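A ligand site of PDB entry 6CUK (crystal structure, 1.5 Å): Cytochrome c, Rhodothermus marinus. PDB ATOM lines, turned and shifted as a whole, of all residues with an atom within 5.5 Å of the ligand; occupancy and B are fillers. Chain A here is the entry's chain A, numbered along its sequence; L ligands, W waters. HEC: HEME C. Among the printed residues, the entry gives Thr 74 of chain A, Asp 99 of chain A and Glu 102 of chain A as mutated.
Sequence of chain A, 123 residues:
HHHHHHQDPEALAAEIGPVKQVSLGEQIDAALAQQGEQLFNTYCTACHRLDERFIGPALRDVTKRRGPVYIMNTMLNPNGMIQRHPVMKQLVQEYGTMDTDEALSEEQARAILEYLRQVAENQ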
ATOM      1  N   PHE A  40      11.876  14.909 -23.696  1.00  0.00           N
ATOM      2  CA  PHE A  40      10.953  13.900 -23.122  1.00  0.00           C
ATOM      3  C   PHE A  40       9.789  13.650 -24.094  1.00  0.00           C
ATOM      4  O   PHE A  40       9.384  12.497 -24.332  1.00  0.00           O
ATOM      5  CB  PHE A  40      10.464  14.381 -21.777  1.00  0.00           C
ATOM      6  CG  PHE A  40       9.616  13.387 -21.025  1.00  0.00           C
ATOM      7  CD1 PHE A  40      10.222  12.411 -20.249  1.00  0.00           C
ATOM      8  CD2 PHE A  40       8.261  13.376 -21.154  1.00  0.00           C
ATOM      9  CE1 PHE A  40       9.462  11.515 -19.531  1.00  0.00           C
ATOM     10  CE2 PHE A  40       7.494  12.435 -20.474  1.00  0.00           C
ATOM     11  CZ  PHE A  40       8.098  11.475 -19.682  1.00  0.00           C
ATOM     12  N   TYR A  43      11.245  11.614 -27.268  1.00  0.00           N
ATOM     13  CA  TYR A  43      11.834  10.286 -27.078  1.00  0.00           C
ATOM     14  C   TYR A  43      11.028   9.426 -26.095  1.00  0.00           C
ATOM     15  O   TYR A  43      10.699   8.278 -26.390  1.00  0.00           O
ATOM     16  CB  TYR A  43      13.305  10.402 -26.665  1.00  0.00           C
ATOM     17  CG  TYR A  43      14.138  10.991 -27.762  1.00  0.00           C
ATOM     18  CD1 TYR A  43      14.316  10.291 -28.954  1.00  0.00           C
ATOM     19  CD2 TYR A  43      14.678  12.266 -27.628  1.00  0.00           C
ATOM     20  CE1 TYR A  43      15.008  10.848 -30.003  1.00  0.00           C
ATOM     21  CE2 TYR A  43      15.428  12.820 -28.690  1.00  0.00           C
ATOM     22  CZ  TYR A  43      15.576  12.105 -29.856  1.00  0.00           C
ATOM     23  OH  TYR A  43      16.282  12.658 -30.932  1.00  0.00           O
ATOM     24  N   CYS A  44      10.616   9.956 -24.983  1.00  0.00           N
ATOM     25  CA  CYS A  44      10.089   9.137 -23.916  1.00  0.00           C
ATOM     26  C   CYS A  44       8.587   8.889 -23.965  1.00  0.00           C
ATOM     27  O   CYS A  44       8.129   7.858 -23.459  1.00  0.00           O
ATOM     28  CB  CYS A  44      10.432   9.726 -22.547  1.00  0.00           C
ATOM     29  SG  CYS A  44      12.169  10.301 -22.434  1.00  0.00           S
ATOM     30  N   ALA A  46       6.886   8.031 -26.400  1.00  0.00           N
ATOM     31  CA  ALA A  46       6.564   6.771 -27.108  1.00  0.00           C
ATOM     32  C   ALA A  46       6.058   5.723 -26.171  1.00  0.00           C
ATOM     33  O   ALA A  46       5.263   4.891 -26.584  1.00  0.00           O
ATOM     34  CB  ALA A  46       7.767   6.218 -27.823  1.00  0.00           C
ATOM     35  N   CYS A  47       6.506   5.734 -24.916  1.00  0.00           N
ATOM     36  CA  CYS A  47       6.175   4.667 -23.967  1.00  0.00           C
ATOM     37  C   CYS A  47       5.704   5.097 -22.602  1.00  0.00           C
ATOM     38  O   CYS A  47       5.104   4.293 -21.863  1.00  0.00           O
ATOM     39  CB  CYS A  47       7.345   3.720 -23.801  1.00  0.00           C
ATOM     40  SG  CYS A  47       7.868   2.972 -25.376  1.00  0.00           S
ATOM     41  N   HIS A  48       5.969   6.339 -22.240  1.00  0.00           N
ATOM     42  CA  HIS A  48       5.662   6.806 -20.889  1.00  0.00           C
ATOM     43  C   HIS A  48       4.712   8.013 -20.857  1.00  0.00           C
ATOM     44  O   HIS A  48       4.712   8.831 -21.802  1.00  0.00           O
ATOM     45  CB  HIS A  48       6.953   7.259 -20.186  1.00  0.00           C
ATOM     46  CG  HIS A  48       7.937   6.160 -19.856  1.00  0.00           C
ATOM     47  ND1 HIS A  48       7.813   5.323 -18.757  1.00  0.00           N
ATOM     48  CD2 HIS A  48       9.111   5.807 -20.462  1.00  0.00           C
ATOM     49  CE1 HIS A  48       8.917   4.558 -18.693  1.00  0.00           C
ATOM     50  NE2 HIS A  48       9.685   4.802 -19.754  1.00  0.00           N
ATOM     51  N   ILE A  55       3.190   2.033 -21.932  1.00  0.00           N
ATOM     52  CA  ILE A  55       4.003   0.912 -22.253  1.00  0.00           C
ATOM     53  C   ILE A  55       4.946   0.666 -21.082  1.00  0.00           C
ATOM     54  O   ILE A  55       5.250  -0.505 -20.751  1.00  0.00           O
ATOM     55  CB  ILE A  55       4.714   1.069 -23.623  1.00  0.00           C
ATOM     56  CG1 ILE A  55       3.674   0.985 -24.795  1.00  0.00           C
ATOM     57  CG2 ILE A  55       5.816   0.038 -23.756  1.00  0.00           C
ATOM     58  CD1 ILE A  55       4.187   1.514 -26.118  1.00  0.00           C
ATOM     59  N   GLY A  56       5.478   1.755 -20.487  1.00  0.00           N
ATOM     60  CA  GLY A  56       6.243   1.683 -19.274  1.00  0.00           C
ATOM     61  C   GLY A  56       5.580   2.388 -18.093  1.00  0.00           C
ATOM     62  O   GLY A  56       4.497   2.960 -18.285  1.00  0.00           O
ATOM     63  N   PRO A  57       6.174   2.364 -16.894  1.00  0.00           N
ATOM     64  CA  PRO A  57       5.577   3.007 -15.724  1.00  0.00           C
ATOM     65  C   PRO A  57       5.419   4.507 -15.867  1.00  0.00           C
ATOM     66  O   PRO A  57       6.216   5.153 -16.569  1.00  0.00           O
ATOM     67  CB  PRO A  57       6.550   2.712 -14.571  1.00  0.00           C
ATOM     68  CG  PRO A  57       7.744   2.142 -15.239  1.00  0.00           C
ATOM     69  CD  PRO A  57       7.351   1.575 -16.531  1.00  0.00           C
ATOM     70  N   ALA A  58       4.452   5.087 -15.151  1.00  0.00           N
ATOM     71  CA  ALA A  58       4.316   6.525 -15.017  1.00  0.00           C
ATOM     72  C   ALA A  58       5.560   7.133 -14.370  1.00  0.00           C
ATOM     73  O   ALA A  58       6.114   6.489 -13.479  1.00  0.00           O
ATOM     74  CB  ALA A  58       3.071   6.848 -14.209  1.00  0.00           C
ATOM     75  N   LEU A  59       5.924   8.352 -14.761  1.00  0.00           N
ATOM     76  CA  LEU A  59       7.193   8.939 -14.331  1.00  0.00           C
ATOM     77  C   LEU A  59       7.131  10.240 -13.589  1.00  0.00           C
ATOM     78  O   LEU A  59       8.166  10.714 -13.139  1.00  0.00           O
ATOM     79  CB  LEU A  59       8.135   9.114 -15.546  1.00  0.00           C
ATOM     80  CG  LEU A  59       8.563   7.842 -16.286  1.00  0.00           C
ATOM     81  CD1 LEU A  59       9.459   8.213 -17.471  1.00  0.00           C
ATOM     82  CD2 LEU A  59       9.253   6.843 -15.343  1.00  0.00           C
ATOM     83  N   VAL A  62       9.085   9.802 -10.400  1.00  0.00           N
ATOM     84  CA  VAL A  62      10.210   8.910 -10.449  1.00  0.00           C
ATOM     85  C   VAL A  62      11.368   9.494  -9.627  1.00  0.00           C
ATOM     86  O   VAL A  62      12.119   8.718  -9.027  1.00  0.00           O
ATOM     87  CB  VAL A  62      10.611   8.550 -11.894  1.00  0.00           C
ATOM     88  CG1 VAL A  62      11.265   9.702 -12.660  1.00  0.00           C
ATOM     89  CG2 VAL A  62      11.574   7.367 -11.867  1.00  0.00           C
ATOM     90  N   ARG A  65      10.898   8.447  -5.881  1.00  0.00           N
ATOM     91  CA  ARG A  65      11.179   7.074  -5.515  1.00  0.00           C
ATOM     92  C   ARG A  65      12.552   6.569  -5.907  1.00  0.00           C
ATOM     93  O   ARG A  65      13.017   5.598  -5.342  1.00  0.00           O
ATOM     94  CB  ARG A  65      10.095   6.130  -6.008  1.00  0.00           C
ATOM     95  CG  ARG A  65       9.876   6.136  -7.505  1.00  0.00           C
ATOM     96  CD  ARG A  65       8.856   5.108  -7.940  1.00  0.00           C
ATOM     97  NE  ARG A  65       8.748   5.078  -9.406  1.00  0.00           N
ATOM     98  CZ  ARG A  65       7.954   5.821 -10.146  1.00  0.00           C
ATOM     99  NH1 ARG A  65       8.016   5.703 -11.475  1.00  0.00           N
ATOM    100  NH2 ARG A  65       7.108   6.696  -9.645  1.00  0.00           N
ATOM    101  N   ARG A  66      13.192   7.202  -6.915  1.00  0.00           N
ATOM    102  CA  ARG A  66      14.560   6.845  -7.359  1.00  0.00           C
ATOM    103  C   ARG A  66      15.494   8.043  -7.230  1.00  0.00           C
ATOM    104  O   ARG A  66      15.042   9.177  -7.137  1.00  0.00           O
ATOM    105  CB  ARG A  66      14.567   6.381  -8.828  1.00  0.00           C
ATOM    106  CG  ARG A  66      13.422   5.460  -9.233  1.00  0.00           C
ATOM    107  CD  ARG A  66      13.418   4.154  -8.486  1.00  0.00           C
ATOM    108  NE  ARG A  66      12.329   3.328  -8.950  1.00  0.00           N
ATOM    109  CZ  ARG A  66      11.605   2.477  -8.236  1.00  0.00           C
ATOM    110  NH1 ARG A  66      11.933   2.240  -6.995  1.00  0.00           N
ATOM    111  NH2 ARG A  66      10.544   1.853  -8.823  1.00  0.00           N
ATOM    112  N   TYR A  70      20.478   6.243 -10.939  1.00  0.00           N
ATOM    113  CA  TYR A  70      19.567   5.260 -11.500  1.00  0.00           C
ATOM    114  C   TYR A  70      18.811   5.797 -12.702  1.00  0.00           C
ATOM    115  O   TYR A  70      18.712   5.110 -13.730  1.00  0.00           O
ATOM    116  CB  TYR A  70      18.592   4.779 -10.413  1.00  0.00           C
ATOM    117  CG  TYR A  70      17.474   3.844 -10.859  1.00  0.00           C
ATOM    118  CD1 TYR A  70      16.286   4.379 -11.381  1.00  0.00           C
ATOM    119  CD2 TYR A  70      17.590   2.474 -10.791  1.00  0.00           C
ATOM    120  CE1 TYR A  70      15.259   3.581 -11.724  1.00  0.00           C
ATOM    121  CE2 TYR A  70      16.571   1.651 -11.172  1.00  0.00           C
ATOM    122  CZ  TYR A  70      15.391   2.224 -11.643  1.00  0.00           C
ATOM    123  OH  TYR A  70      14.324   1.414 -12.046  1.00  0.00           O
ATOM    124  N   ILE A  71      18.257   6.990 -12.605  1.00  0.00           N
ATOM    125  CA  ILE A  71      17.490   7.551 -13.699  1.00  0.00           C
ATOM    126  C   ILE A  71      18.423   7.795 -14.887  1.00  0.00           C
ATOM    127  O   ILE A  71      18.049   7.465 -16.029  1.00  0.00           O
ATOM    128  CB  ILE A  71      16.733   8.832 -13.254  1.00  0.00           C
ATOM    129  CG1 ILE A  71      15.686   8.481 -12.200  1.00  0.00           C
ATOM    130  CG2 ILE A  71      16.127   9.567 -14.459  1.00  0.00           C
ATOM    131  CD1 ILE A  71      15.106   9.688 -11.500  1.00  0.00           C
ATOM    132  N   THR A  74      19.395   4.494 -16.530  1.00  0.00           N
ATOM    133  CA  THR A  74      18.250   3.928 -17.281  1.00  0.00           C
ATOM    134  C   THR A  74      18.208   4.488 -18.684  1.00  0.00           C
ATOM    135  O   THR A  74      18.001   3.737 -19.643  1.00  0.00           O
ATOM    136  CB  THR A  74      16.965   4.157 -16.470  1.00  0.00           C
ATOM    137  OG1 THR A  74      17.020   3.408 -15.257  1.00  0.00           O
ATOM    138  CG2 THR A  74      15.755   3.751 -17.328  1.00  0.00           C
ATOM    139  N   MET A  75      18.467   5.794 -18.821  1.00  0.00           N
ATOM    140  CA  MET A  75      18.509   6.404 -20.149  1.00  0.00           C
ATOM    141  C   MET A  75      19.729   6.061 -20.989  1.00  0.00           C
ATOM    142  O   MET A  75      19.675   5.905 -22.212  1.00  0.00           O
ATOM    143  CB  MET A  75      18.393   7.929 -20.068  1.00  0.00           C
ATOM    144  CG  MET A  75      17.002   8.403 -19.635  1.00  0.00           C
ATOM    145  SD  MET A  75      16.923  10.231 -19.650  1.00  0.00           S
ATOM    146  CE  MET A  75      17.151  10.562 -17.945  1.00  0.00           C
ATOM    147  N   ILE A  82      18.649  -3.222 -17.027  1.00  0.00           N
ATOM    148  CA  ILE A  82      17.749  -4.354 -17.157  1.00  0.00           C
ATOM    149  C   ILE A  82      18.431  -5.671 -16.737  1.00  0.00           C
ATOM    150  O   ILE A  82      17.793  -6.510 -16.061  1.00  0.00           O
ATOM    151  CB  ILE A  82      17.210  -4.439 -18.634  1.00  0.00           C
ATOM    152  CG1 ILE A  82      16.179  -3.327 -18.892  1.00  0.00           C
ATOM    153  CG2 ILE A  82      16.627  -5.801 -18.968  1.00  0.00           C
ATOM    154  CD1 ILE A  82      16.012  -2.967 -20.358  1.00  0.00           C
ATOM    155  N   VAL A  87      15.885  -3.373  -9.184  1.00  0.00           N
ATOM    156  CA  VAL A  87      14.639  -2.633  -9.307  1.00  0.00           C
ATOM    157  C   VAL A  87      14.201  -2.717 -10.742  1.00  0.00           C
ATOM    158  O   VAL A  87      13.010  -2.966 -11.016  1.00  0.00           O
ATOM    159  CB  VAL A  87      14.798  -1.148  -8.897  1.00  0.00           C
ATOM    160  CG1 VAL A  87      13.525  -0.396  -9.187  1.00  0.00           C
ATOM    161  CG2 VAL A  87      15.183  -1.025  -7.423  1.00  0.00           C
ATOM    162  N   MET A  88      15.149  -2.528 -11.674  1.00  0.00           N
ATOM    163  CA  MET A  88      14.817  -2.598 -13.084  1.00  0.00           C
ATOM    164  C   MET A  88      14.452  -4.017 -13.529  1.00  0.00           C
ATOM    165  O   MET A  88      13.472  -4.190 -14.243  1.00  0.00           O
ATOM    166  CB  MET A  88      15.945  -2.023 -13.951  1.00  0.00           C
ATOM    167  CG  MET A  88      15.564  -1.813 -15.377  1.00  0.00           C
ATOM    168  SD  MET A  88      14.235  -0.654 -15.626  1.00  0.00           S
ATOM    169  CE  MET A  88      15.015   0.899 -15.588  1.00  0.00           C
ATOM    170  N   LEU A  91      10.944  -4.598 -12.764  1.00  0.00           N
ATOM    171  CA  LEU A  91      10.048  -3.937 -13.675  1.00  0.00           C
ATOM    172  C   LEU A  91       9.964  -4.616 -15.032  1.00  0.00           C
ATOM    173  O   LEU A  91       8.901  -4.534 -15.676  1.00  0.00           O
ATOM    174  CB  LEU A  91      10.519  -2.493 -13.904  1.00  0.00           C
ATOM    175  CG  LEU A  91      10.404  -1.572 -12.700  1.00  0.00           C
ATOM    176  CD1 LEU A  91      11.162  -0.251 -13.014  1.00  0.00           C
ATOM    177  CD2 LEU A  91       8.982  -1.298 -12.335  1.00  0.00           C
ATOM    178  N   VAL A  92      11.035  -5.244 -15.492  1.00  0.00           N
ATOM    179  CA  VAL A  92      11.024  -5.984 -16.757  1.00  0.00           C
ATOM    180  C   VAL A  92      10.101  -7.208 -16.733  1.00  0.00           C
ATOM    181  O   VAL A  92       9.445  -7.504 -17.732  1.00  0.00           O
ATOM    182  CB  VAL A  92      12.444  -6.441 -17.174  1.00  0.00           C
ATOM    183  CG1 VAL A  92      12.438  -7.359 -18.402  1.00  0.00           C
ATOM    184  CG2 VAL A  92      13.292  -5.203 -17.456  1.00  0.00           C
ATOM    185  N   GLN A  93      10.086  -7.897 -15.628  1.00  0.00           N
ATOM    186  CA  GLN A  93       9.195  -9.050 -15.452  1.00  0.00           C
ATOM    187  C   GLN A  93       7.729  -8.596 -15.540  1.00  0.00           C
ATOM    188  O   GLN A  93       6.903  -9.310 -16.066  1.00  0.00           O
ATOM    189  CB  GLN A  93       9.512  -9.790 -14.153  1.00  0.00           C
ATOM    190  CG  GLN A  93      10.794 -10.644 -14.224  1.00  0.00           C
ATOM    191  CD  GLN A  93      10.885 -11.447 -15.534  1.00  0.00           C
ATOM    192  OE1 GLN A  93      10.030 -12.295 -15.809  1.00  0.00           O
ATOM    193  NE2 GLN A  93      11.889 -11.145 -16.372  1.00  0.00           N
ATOM    194  N   TYR A  95       6.595  -5.377 -17.088  1.00  0.00           N
ATOM    195  CA  TYR A  95       6.258  -4.603 -18.282  1.00  0.00           C
ATOM    196  C   TYR A  95       6.739  -5.195 -19.586  1.00  0.00           C
ATOM    197  O   TYR A  95       6.289  -4.730 -20.627  1.00  0.00           O
ATOM    198  CB  TYR A  95       6.784  -3.155 -18.163  1.00  0.00           C
ATOM    199  CG  TYR A  95       6.094  -2.308 -17.139  1.00  0.00           C
ATOM    200  CD1 TYR A  95       5.024  -1.521 -17.494  1.00  0.00           C
ATOM    201  CD2 TYR A  95       6.525  -2.282 -15.812  1.00  0.00           C
ATOM    202  CE1 TYR A  95       4.402  -0.707 -16.577  1.00  0.00           C
ATOM    203  CE2 TYR A  95       5.909  -1.505 -14.890  1.00  0.00           C
ATOM    204  CZ  TYR A  95       4.834  -0.726 -15.280  1.00  0.00           C
ATOM    205  OH  TYR A  95       4.204   0.085 -14.412  1.00  0.00           O
ATOM    206  N   GLY A  96       7.683  -6.139 -19.564  1.00  0.00           N
ATOM    207  CA  GLY A  96       8.143  -6.828 -20.774  1.00  0.00           C
ATOM    208  C   GLY A  96       9.467  -6.303 -21.320  1.00  0.00           C
ATOM    209  O   GLY A  96      10.015  -5.295 -20.814  1.00  0.00           O
ATOM    210  N   THR A  97       9.965  -6.997 -22.344  1.00  0.00           N
ATOM    211  CA  THR A  97      11.267  -6.754 -22.959  1.00  0.00           C
ATOM    212  C   THR A  97      11.089  -6.120 -24.326  1.00  0.00           C
ATOM    213  O   THR A  97      10.481  -6.687 -25.210  1.00  0.00           O
ATOM    214  CB  THR A  97      12.058  -8.068 -23.122  1.00  0.00           C
ATOM    215  OG1 THR A  97      12.105  -8.756 -21.870  1.00  0.00           O
ATOM    216  CG2 THR A  97      13.493  -7.818 -23.559  1.00  0.00           C
ATOM    217  N   MET A  98      11.674  -4.955 -24.503  1.00  0.00           N
ATOM    218  CA  MET A  98      11.585  -4.203 -25.753  1.00  0.00           C
ATOM    219  C   MET A  98      12.803  -3.328 -25.872  1.00  0.00           C
ATOM    220  O   MET A  98      13.523  -3.129 -24.886  1.00  0.00           O
ATOM    221  CB  MET A  98      10.334  -3.340 -25.767  1.00  0.00           C
ATOM    222  CG  MET A  98      10.218  -2.370 -24.586  1.00  0.00           C
ATOM    223  SD  MET A  98       8.560  -1.706 -24.479  1.00  0.00           S
ATOM    224  CE  MET A  98       7.702  -3.184 -23.889  1.00  0.00           C
ATOM    225  N   ASP A  99      13.050  -2.782 -27.054  1.00  0.00           N
ATOM    226  CA  ASP A  99      14.183  -1.871 -27.269  1.00  0.00           C
ATOM    227  C   ASP A  99      13.794  -0.484 -26.736  1.00  0.00           C
ATOM    228  O   ASP A  99      12.969   0.219 -27.312  1.00  0.00           O
ATOM    229  CB  ASP A  99      14.583  -1.818 -28.753  1.00  0.00           C
ATOM    230  CG  ASP A  99      15.921  -1.078 -28.994  1.00  0.00           C
ATOM    231  OD1 ASP A  99      16.460  -0.431 -28.067  1.00  0.00           O
ATOM    232  OD2 ASP A  99      16.438  -1.138 -30.130  1.00  0.00           O
ATOM    233  N   THR A 100      14.400  -0.098 -25.602  1.00  0.00           N
ATOM    234  CA  THR A 100      14.089   1.196 -24.984  1.00  0.00           C
ATOM    235  C   THR A 100      15.206   2.230 -25.216  1.00  0.00           C
ATOM    236  O   THR A 100      15.053   3.390 -24.825  1.00  0.00           O
ATOM    237  CB  THR A 100      13.872   1.044 -23.473  1.00  0.00           C
ATOM    238  OG1 THR A 100      15.099   0.590 -22.857  1.00  0.00           O
ATOM    239  CG2 THR A 100      12.766   0.024 -23.139  1.00  0.00           C
ATOM    240  N   GLU A 102      17.310   4.966 -26.693  1.00  0.00           N
ATOM    241  CA  GLU A 102      17.083   6.121 -27.552  1.00  0.00           C
ATOM    242  C   GLU A 102      18.416   6.757 -28.043  1.00  0.00           C
ATOM    243  O   GLU A 102      18.371   7.814 -28.667  1.00  0.00           O
ATOM    244  CB  GLU A 102      16.242   7.140 -26.758  1.00  0.00           C
ATOM    245  CG  GLU A 102      14.808   6.692 -26.460  1.00  0.00           C
ATOM    246  CD  GLU A 102      13.950   6.703 -27.714  1.00  0.00           C
ATOM    247  OE1 GLU A 102      14.533   6.750 -28.807  1.00  0.00           O
ATOM    248  OE2 GLU A 102      12.719   6.718 -27.615  1.00  0.00           O
ATOM    249  N   LEU A 104      20.739   8.397 -26.494  1.00  0.00           N
ATOM    250  CA  LEU A 104      20.863   9.750 -26.005  1.00  0.00           C
ATOM    251  C   LEU A 104      22.267  10.040 -25.613  1.00  0.00           C
ATOM    252  O   LEU A 104      23.011   9.142 -25.208  1.00  0.00           O
ATOM    253  CB  LEU A 104      19.997   9.960 -24.752  1.00  0.00           C
ATOM    254  CG  LEU A 104      18.516   9.852 -24.907  1.00  0.00           C
ATOM    255  CD1 LEU A 104      17.962  10.117 -23.517  1.00  0.00           C
ATOM    256  CD2 LEU A 104      17.910  10.791 -25.892  1.00  0.00           C
ATOM    257  N   ILE A 112      16.738  15.853 -19.540  1.00  0.00           N
ATOM    258  CA  ILE A 112      15.530  15.094 -19.189  1.00  0.00           C
ATOM    259  C   ILE A 112      15.378  14.880 -17.688  1.00  0.00           C
ATOM    260  O   ILE A 112      14.323  15.041 -17.098  1.00  0.00           O
ATOM    261  CB  ILE A 112      15.446  13.779 -19.945  1.00  0.00           C
ATOM    262  CG1 ILE A 112      15.268  14.066 -21.447  1.00  0.00           C
ATOM    263  CG2 ILE A 112      14.290  12.909 -19.431  1.00  0.00           C
ATOM    264  CD1 ILE A 112      15.447  12.823 -22.308  1.00  0.00           C
ATOM    265  N   LEU A 116      12.278  15.903 -15.295  1.00  0.00           N
ATOM    266  CA  LEU A 116      11.655  14.977 -14.323  1.00  0.00           C
ATOM    267  C   LEU A 116      11.651  15.551 -12.919  1.00  0.00           C
ATOM    268  O   LEU A 116      10.710  15.370 -12.159  1.00  0.00           O
ATOM    269  CB  LEU A 116      12.280  13.611 -14.377  1.00  0.00           C
ATOM    270  CG  LEU A 116      12.046  12.851 -15.694  1.00  0.00           C
ATOM    271  CD1 LEU A 116      12.959  11.642 -15.828  1.00  0.00           C
ATOM    272  CD2 LEU A 116      10.565  12.528 -15.838  1.00  0.00           C
HETATM  273 FE   HEC L   1      11.487   3.989 -20.006  1.00  0.00          FE
HETATM  274  CHA HEC L   1      11.267   2.032 -17.221  1.00  0.00           C
HETATM  275  CHB HEC L   1      12.765   6.522 -18.127  1.00  0.00           C
HETATM  276  CHC HEC L   1      12.124   5.775 -22.853  1.00  0.00           C
HETATM  277  CHD HEC L   1       9.746   1.683 -21.834  1.00  0.00           C
HETATM  278  NA  HEC L   1      11.948   4.208 -18.061  1.00  0.00           N
HETATM  279  C1A HEC L   1      11.769   3.303 -17.024  1.00  0.00           C
HETATM  280  C2A HEC L   1      12.249   3.868 -15.786  1.00  0.00           C
HETATM  281  C3A HEC L   1      12.680   5.127 -16.074  1.00  0.00           C
HETATM  282  C4A HEC L   1      12.475   5.354 -17.485  1.00  0.00           C
HETATM  283  CMA HEC L   1      13.302   6.165 -15.113  1.00  0.00           C
HETATM  284  CAA HEC L   1      12.240   3.141 -14.416  1.00  0.00           C
HETATM  285  CBA HEC L   1      11.006   3.638 -13.648  1.00  0.00           C
HETATM  286  CGA HEC L   1      10.990   3.272 -12.175  1.00  0.00           C
HETATM  287  O1A HEC L   1       9.951   3.458 -11.502  1.00  0.00           O
HETATM  288  O2A HEC L   1      12.065   2.892 -11.632  1.00  0.00           O
HETATM  289  NB  HEC L   1      12.303   5.768 -20.412  1.00  0.00           N
HETATM  290  C1B HEC L   1      12.649   6.732 -19.472  1.00  0.00           C
HETATM  291  C2B HEC L   1      12.954   7.953 -20.153  1.00  0.00           C
HETATM  292  C3B HEC L   1      12.800   7.776 -21.476  1.00  0.00           C
HETATM  293  C4B HEC L   1      12.374   6.408 -21.654  1.00  0.00           C
HETATM  294  CMB HEC L   1      13.365   9.236 -19.430  1.00  0.00           C
HETATM  295  CAB HEC L   1      12.999   8.830 -22.590  1.00  0.00           C
HETATM  296  CBB HEC L   1      14.518   9.135 -22.703  1.00  0.00           C
HETATM  297  NC  HEC L   1      11.042   3.773 -21.967  1.00  0.00           N
HETATM  298  C1C HEC L   1      11.428   4.603 -22.998  1.00  0.00           C
HETATM  299  C2C HEC L   1      10.862   4.117 -24.231  1.00  0.00           C
HETATM  300  C3C HEC L   1      10.177   2.969 -23.945  1.00  0.00           C
HETATM  301  C4C HEC L   1      10.296   2.733 -22.549  1.00  0.00           C
HETATM  302  CMC HEC L   1      10.993   4.767 -25.599  1.00  0.00           C
HETATM  303  CAC HEC L   1       9.276   2.117 -24.932  1.00  0.00           C
HETATM  304  CBC HEC L   1      10.059   1.540 -26.079  1.00  0.00           C
HETATM  305  ND  HEC L   1      10.673   2.188 -19.605  1.00  0.00           N
HETATM  306  C1D HEC L   1      10.002   1.390 -20.529  1.00  0.00           C
HETATM  307  C2D HEC L   1       9.693   0.178 -19.845  1.00  0.00           C
HETATM  308  C3D HEC L   1      10.108   0.266 -18.580  1.00  0.00           C
HETATM  309  C4D HEC L   1      10.745   1.551 -18.400  1.00  0.00           C
HETATM  310  CMD HEC L   1       8.931  -0.975 -20.531  1.00  0.00           C
HETATM  311  CAD HEC L   1       9.982  -0.784 -17.452  1.00  0.00           C
HETATM  312  CBD HEC L   1      11.194  -1.715 -17.558  1.00  0.00           C
HETATM  313  CGD HEC L   1      11.138  -2.637 -18.753  1.00  0.00           C
HETATM  314  O1D HEC L   1      10.146  -3.449 -18.827  1.00  0.00           O
HETATM  315  O2D HEC L   1      12.025  -2.585 -19.622  1.00  0.00           O
HETATM  316  O   HOH W   1      15.501   4.770 -21.150  1.00  0.00           O
HETATM  317  O   HOH W   2      13.336   3.058 -20.202  1.00  0.00           O
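The backbone carbonyl oxygen (O) of Gly 96 lies close to an oxygen (O1D) of the ligand, at 2.7 Å.
The guanidinium group of Arg 66 lies within salt-bridge range of an oxygen (O2A) of the ligand, 2.7 Å away.
The side-chain sulfur (SG) of Cys 47 is covalently linked to a carbon (CAC) of the ligand (1.7 Å).
O2A of the ligand lies within hydrogen-bond range of OH of Tyr 70 (2.7 Å).
The guanidinium group (NE) of Arg 65 lies within salt-bridge range of an oxygen (O1A) of the ligand (2.9 Å).
The side-chain sulfur of Cys 44 is covalently linked to a carbon (CAB) of the ligand (1.7 Å).
A ring nitrogen (NE2) of His 48 is bound to an iron atom (FE) of the ligand (2.0 Å).
NH1 of Arg 65 is in hydrogen-bond range of O of Ala 58, 2.9 Å away.
O of Cys 47 lies within hydrogen-bond range of N of Ile 55 (3.0 Å).
A ring nitrogen (ND1) of His 48 sits at hydrogen-bond distance from the backbone carbonyl oxygen of Pro 57 (2.7 Å).
O of Cys 47 sits at hydrogen-bond distance from N of Gly 56, at 2.9 Å.
O of Tyr 70 is in hydrogen-bond range of OG1 of Thr 74 (2.8 Å).
O of Tyr 43 touches CMC of the ligand, at 3.6 Å.
Ile 55 touches the ligand (O to CMD, 3.7 Å).
Gly 56 touches the ligand.
Pro 57 touches the ligand (CD to CAD, 3.7 Å).
Leu 59 touches the ligand (CD1 to CHB, 3.8 Å).
Val 62 touches the ligand (CG2 to CMA, 3.9 Å).
Thr 74 touches the ligand.
Met 75 touches the ligand.
Met 88 touches the ligand.
Leu 91 touches the ligand (CD1 to O2A, 3.6 Å).
Val 92 touches the ligand.
Tyr 95 touches the ligand.
SD of Met 98 touches CAC of the ligand, 3.9 Å away.
O of Asp 99 touches CBC of the ligand (3.4 Å).
CG2 of Thr 100 touches CHD of the ligand, 3.7 Å away.
Glu 102 touches the ligand (OE2 to CMC, 3.3 Å).
CD1 of Leu 104 touches CBB of the ligand (3.7 Å).
CG2 of Ile 112 touches CMB of the ligand, 3.8 Å away.
Hydrophobic or aromatic side chains that line the ligand: His 48, Pro 57, Leu 59, Val 62, Tyr 70, Met 75, Met 88, Leu 91, Val 92, Tyr 95, Met 98, Leu 104 and Ile 112.
The nearest printed residue that does not touch the ligand is Ile 82 (4.1 Å).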
